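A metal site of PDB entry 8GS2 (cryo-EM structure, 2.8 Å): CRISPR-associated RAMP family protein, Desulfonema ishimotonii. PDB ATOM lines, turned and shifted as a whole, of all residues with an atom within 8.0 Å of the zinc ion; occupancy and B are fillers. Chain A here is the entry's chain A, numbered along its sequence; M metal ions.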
ATOM      1  N   ARG A 452      10.908  -3.490  -0.518  1.00  0.00           N
ATOM      2  CA  ARG A 452      11.249  -3.196   0.878  1.00  0.00           C
ATOM      3  C   ARG A 452       9.991  -3.019   1.718  1.00  0.00           C
ATOM      4  O   ARG A 452       9.914  -3.504   2.853  1.00  0.00           O
ATOM      5  CB  ARG A 452      12.128  -1.952   0.945  1.00  0.00           C
ATOM      6  CG  ARG A 452      12.550  -1.559   2.350  1.00  0.00           C
ATOM      7  CD  ARG A 452      13.409  -0.310   2.335  1.00  0.00           C
ATOM      8  NE  ARG A 452      14.675  -0.535   1.656  1.00  0.00           N
ATOM      9  CZ  ARG A 452      15.778  -0.968   2.244  1.00  0.00           C
ATOM     10  NH1 ARG A 452      15.801  -1.265   3.533  1.00  0.00           N
ATOM     11  NH2 ARG A 452      16.884  -1.121   1.526  1.00  0.00           N
ATOM     12  N   GLN A 456       8.967  -5.397   4.886  1.00  0.00           N
ATOM     13  CA  GLN A 456       8.647  -4.865   6.205  1.00  0.00           C
ATOM     14  C   GLN A 456       7.236  -5.240   6.641  1.00  0.00           C
ATOM     15  O   GLN A 456       7.000  -5.484   7.832  1.00  0.00           O
ATOM     16  CB  GLN A 456       8.821  -3.346   6.224  1.00  0.00           C
ATOM     17  CG  GLN A 456      10.259  -2.887   6.058  1.00  0.00           C
ATOM     18  CD  GLN A 456      10.374  -1.383   6.059  1.00  0.00           C
ATOM     19  OE1 GLN A 456      10.623  -0.768   7.099  1.00  0.00           O
ATOM     20  NE2 GLN A 456      10.211  -0.777   4.896  1.00  0.00           N
ATOM     21  N   SER A 461       7.653  -5.321  11.127  1.00  0.00           N
ATOM     22  CA  SER A 461       8.623  -4.553  11.910  1.00  0.00           C
ATOM     23  C   SER A 461       9.223  -3.475  11.033  1.00  0.00           C
ATOM     24  O   SER A 461      10.085  -3.777  10.189  1.00  0.00           O
ATOM     25  CB  SER A 461       9.711  -5.453  12.478  1.00  0.00           C
ATOM     26  OG  SER A 461      10.428  -6.100  11.449  1.00  0.00           O
ATOM     27  N   PRO A 462       8.807  -2.214  11.181  1.00  0.00           N
ATOM     28  CA  PRO A 462       9.382  -1.139  10.363  1.00  0.00           C
ATOM     29  C   PRO A 462      10.865  -0.970  10.653  1.00  0.00           C
ATOM     30  O   PRO A 462      11.337  -1.188  11.765  1.00  0.00           O
ATOM     31  CB  PRO A 462       8.587   0.104  10.784  1.00  0.00           C
ATOM     32  CG  PRO A 462       7.331  -0.441  11.395  1.00  0.00           C
ATOM     33  CD  PRO A 462       7.721  -1.723  12.042  1.00  0.00           C
ATOM     34  N   CYS A 463      11.599  -0.558   9.625  1.00  0.00           N
ATOM     35  CA  CYS A 463      13.029  -0.279   9.748  1.00  0.00           C
ATOM     36  C   CYS A 463      13.201   1.199  10.055  1.00  0.00           C
ATOM     37  O   CYS A 463      13.109   2.053   9.159  1.00  0.00           O
ATOM     38  CB  CYS A 463      13.771  -0.679   8.475  1.00  0.00           C
ATOM     39  SG  CYS A 463      15.527  -0.267   8.512  1.00  0.00           S
ATOM     40  N   ASN A 464      13.434   1.518  11.326  1.00  0.00           N
ATOM     41  CA  ASN A 464      13.613   2.903  11.752  1.00  0.00           C
ATOM     42  C   ASN A 464      15.091   3.300  11.700  1.00  0.00           C
ATOM     43  O   ASN A 464      15.712   3.647  12.700  1.00  0.00           O
ATOM     44  CB  ASN A 464      13.034   3.093  13.155  1.00  0.00           C
ATOM     45  CG  ASN A 464      11.535   2.855  13.207  1.00  0.00           C
ATOM     46  OD1 ASN A 464      10.809   3.180  12.267  1.00  0.00           O
ATOM     47  ND2 ASN A 464      11.069   2.276  14.297  1.00  0.00           N
ATOM     48  N   ALA A 465      15.632   3.232  10.491  1.00  0.00           N
ATOM     49  CA  ALA A 465      17.019   3.587  10.236  1.00  0.00           C
ATOM     50  C   ALA A 465      17.099   4.928   9.519  1.00  0.00           C
ATOM     51  O   ALA A 465      16.111   5.420   8.968  1.00  0.00           O
ATOM     52  CB  ALA A 465      17.711   2.507   9.398  1.00  0.00           C
ATOM     53  N   GLU A 466      18.293   5.508   9.551  1.00  0.00           N
ATOM     54  CA  GLU A 466      18.547   6.799   8.930  1.00  0.00           C
ATOM     55  C   GLU A 466      19.715   6.680   7.961  1.00  0.00           C
ATOM     56  O   GLU A 466      20.598   5.838   8.125  1.00  0.00           O
ATOM     57  CB  GLU A 466      18.847   7.871   9.993  1.00  0.00           C
ATOM     58  CG  GLU A 466      18.984   9.291   9.465  1.00  0.00           C
ATOM     59  CD  GLU A 466      17.706   9.803   8.822  1.00  0.00           C
ATOM     60  OE1 GLU A 466      16.605   9.340   9.220  1.00  0.00           O
ATOM     61  OE2 GLU A 466      17.792  10.660   7.924  1.00  0.00           O
ATOM     62  N   PRO A 471      26.048  -0.084   7.788  1.00  0.00           N
ATOM     63  CA  PRO A 471      24.827  -0.668   7.231  1.00  0.00           C
ATOM     64  C   PRO A 471      23.900  -1.216   8.313  1.00  0.00           C
ATOM     65  O   PRO A 471      24.341  -1.762   9.314  1.00  0.00           O
ATOM     66  CB  PRO A 471      25.361  -1.798   6.341  1.00  0.00           C
ATOM     67  CG  PRO A 471      26.733  -1.365   5.982  1.00  0.00           C
ATOM     68  CD  PRO A 471      27.260  -0.652   7.186  1.00  0.00           C
ATOM     69  N   CYS A 472      22.602  -1.045   8.087  1.00  0.00           N
ATOM     70  CA  CYS A 472      21.607  -1.569   8.999  1.00  0.00           C
ATOM     71  C   CYS A 472      21.603  -3.090   8.982  1.00  0.00           C
ATOM     72  O   CYS A 472      21.735  -3.715   7.919  1.00  0.00           O
ATOM     73  CB  CYS A 472      20.217  -1.042   8.641  1.00  0.00           C
ATOM     74  SG  CYS A 472      18.890  -1.598   9.724  1.00  0.00           S
ATOM     75  N   MET A 473      21.461  -3.694  10.150  1.00  0.00           N
ATOM     76  CA  MET A 473      21.534  -5.146  10.301  1.00  0.00           C
ATOM     77  C   MET A 473      20.166  -5.788  10.495  1.00  0.00           C
ATOM     78  O   MET A 473      20.083  -6.959  10.880  1.00  0.00           O
ATOM     79  CB  MET A 473      22.460  -5.506  11.466  1.00  0.00           C
ATOM     80  CG  MET A 473      23.880  -5.006  11.293  1.00  0.00           C
ATOM     81  SD  MET A 473      24.631  -5.544   9.753  1.00  0.00           S
ATOM     82  CE  MET A 473      24.468  -7.321   9.901  1.00  0.00           C
ATOM     83  N   CYS A 474      19.088  -5.050  10.238  1.00  0.00           N
ATOM     84  CA  CYS A 474      17.767  -5.642  10.329  1.00  0.00           C
ATOM     85  C   CYS A 474      17.561  -6.621   9.171  1.00  0.00           C
ATOM     86  O   CYS A 474      18.227  -6.560   8.137  1.00  0.00           O
ATOM     87  CB  CYS A 474      16.681  -4.575  10.321  1.00  0.00           C
ATOM     88  SG  CYS A 474      16.156  -4.021   8.689  1.00  0.00           S
ATOM     89  N   LYS A 475      16.617  -7.542   9.367  1.00  0.00           N
ATOM     90  CA  LYS A 475      16.410  -8.614   8.395  1.00  0.00           C
ATOM     91  C   LYS A 475      15.969  -8.074   7.041  1.00  0.00           C
ATOM     92  O   LYS A 475      16.398  -8.593   5.999  1.00  0.00           O
ATOM     93  CB  LYS A 475      15.392  -9.622   8.931  1.00  0.00           C
ATOM     94  CG  LYS A 475      14.442  -9.037   9.970  1.00  0.00           C
ATOM     95  CD  LYS A 475      13.697 -10.123  10.716  1.00  0.00           C
ATOM     96  CE  LYS A 475      12.769  -9.539  11.765  1.00  0.00           C
ATOM     97  NZ  LYS A 475      12.006 -10.572  12.496  1.00  0.00           N
ATOM     98  N   THR A 476      15.122  -7.039   7.024  1.00  0.00           N
ATOM     99  CA  THR A 476      14.700  -6.451   5.758  1.00  0.00           C
ATOM    100  C   THR A 476      15.875  -5.869   4.993  1.00  0.00           C
ATOM    101  O   THR A 476      16.018  -6.096   3.784  1.00  0.00           O
ATOM    102  CB  THR A 476      13.632  -5.389   6.004  1.00  0.00           C
ATOM    103  OG1 THR A 476      12.533  -5.954   6.716  1.00  0.00           O
ATOM    104  CG2 THR A 476      13.135  -4.817   4.697  1.00  0.00           C
ATOM    105  N   CYS A 477      16.737  -5.118   5.688  1.00  0.00           N
ATOM    106  CA  CYS A 477      17.913  -4.548   5.028  1.00  0.00           C
ATOM    107  C   CYS A 477      18.900  -5.628   4.597  1.00  0.00           C
ATOM    108  O   CYS A 477      19.519  -5.508   3.532  1.00  0.00           O
ATOM    109  CB  CYS A 477      18.601  -3.546   5.945  1.00  0.00           C
ATOM    110  SG  CYS A 477      17.799  -1.933   6.034  1.00  0.00           S
ATOM    111  N   ARG A 478      19.060  -6.677   5.410  1.00  0.00           N
ATOM    112  CA  ARG A 478      19.934  -7.779   5.015  1.00  0.00           C
ATOM    113  C   ARG A 478      19.434  -8.454   3.747  1.00  0.00           C
ATOM    114  O   ARG A 478      20.232  -8.790   2.862  1.00  0.00           O
ATOM    115  CB  ARG A 478      20.044  -8.796   6.155  1.00  0.00           C
ATOM    116  CG  ARG A 478      20.967  -8.369   7.278  1.00  0.00           C
ATOM    117  CD  ARG A 478      21.089  -9.480   8.311  1.00  0.00           C
ATOM    118  NE  ARG A 478      19.870  -9.614   9.095  1.00  0.00           N
ATOM    119  CZ  ARG A 478      19.547 -10.699   9.788  1.00  0.00           C
ATOM    120  NH1 ARG A 478      20.312 -11.776   9.787  1.00  0.00           N
ATOM    121  NH2 ARG A 478      18.413 -10.703  10.499  1.00  0.00           N
ATOM    122  N   MET A 480      17.502  -6.984   1.449  1.00  0.00           N
ATOM    123  CA  MET A 480      17.547  -6.028   0.351  1.00  0.00           C
ATOM    124  C   MET A 480      18.972  -5.818  -0.157  1.00  0.00           C
ATOM    125  O   MET A 480      19.149  -5.522  -1.344  1.00  0.00           O
ATOM    126  CB  MET A 480      16.946  -4.689   0.778  1.00  0.00           C
ATOM    127  CG  MET A 480      15.442  -4.735   0.998  1.00  0.00           C
ATOM    128  SD  MET A 480      14.535  -5.245  -0.469  1.00  0.00           S
ATOM    129  CE  MET A 480      14.982  -3.961  -1.620  1.00  0.00           C
ATOM    130  N   ARG A 481      19.979  -5.960   0.700  1.00  0.00           N
ATOM    131  CA  ARG A 481      21.355  -5.788   0.245  1.00  0.00           C
ATOM    132  C   ARG A 481      21.794  -6.883  -0.727  1.00  0.00           C
ATOM    133  O   ARG A 481      22.804  -6.704  -1.410  1.00  0.00           O
ATOM    134  CB  ARG A 481      22.306  -5.734   1.434  1.00  0.00           C
ATOM    135  CG  ARG A 481      22.312  -4.398   2.156  1.00  0.00           C
ATOM    136  CD  ARG A 481      23.561  -4.217   3.003  1.00  0.00           C
ATOM    137  NE  ARG A 481      23.654  -5.206   4.068  1.00  0.00           N
ATOM    138  CZ  ARG A 481      23.187  -5.037   5.297  1.00  0.00           C
ATOM    139  NH1 ARG A 481      22.582  -3.921   5.652  1.00  0.00           N
ATOM    140  NH2 ARG A 481      23.332  -6.012   6.196  1.00  0.00           N
HETATM  141 ZN    ZN M   1      17.114  -1.944   8.250  1.00  0.00          ZN
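The side-chain sulfur (SG) of Cys 477 sits close to the guanidinium group (NH1) of Arg 452, 3.3 Å away.
The backbone NH (N) of Cys 463 lies within hydrogen-bond range of the side-chain amide oxygen (OE1) of Gln 456, at 2.7 Å.
The side-chain sulfur (SG) of Cys 474 lies close to the backbone NH (N) of Thr 476, at 3.6 Å.
The guanidinium group (NH1) of Arg 481 lies within hydrogen-bond range of the backbone carbonyl oxygen (O) of Cys 472, at 2.4 Å.
Of the 18 residues printed, 4 come within 4 Å of the zinc ion.
The zinc ion is bound by SG of Cys 477 (2.3 Å), SG of Cys 463 (2.3 Å), SG of Cys 474 (2.3 Å) and SG of Cys 472 (2.3 Å).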
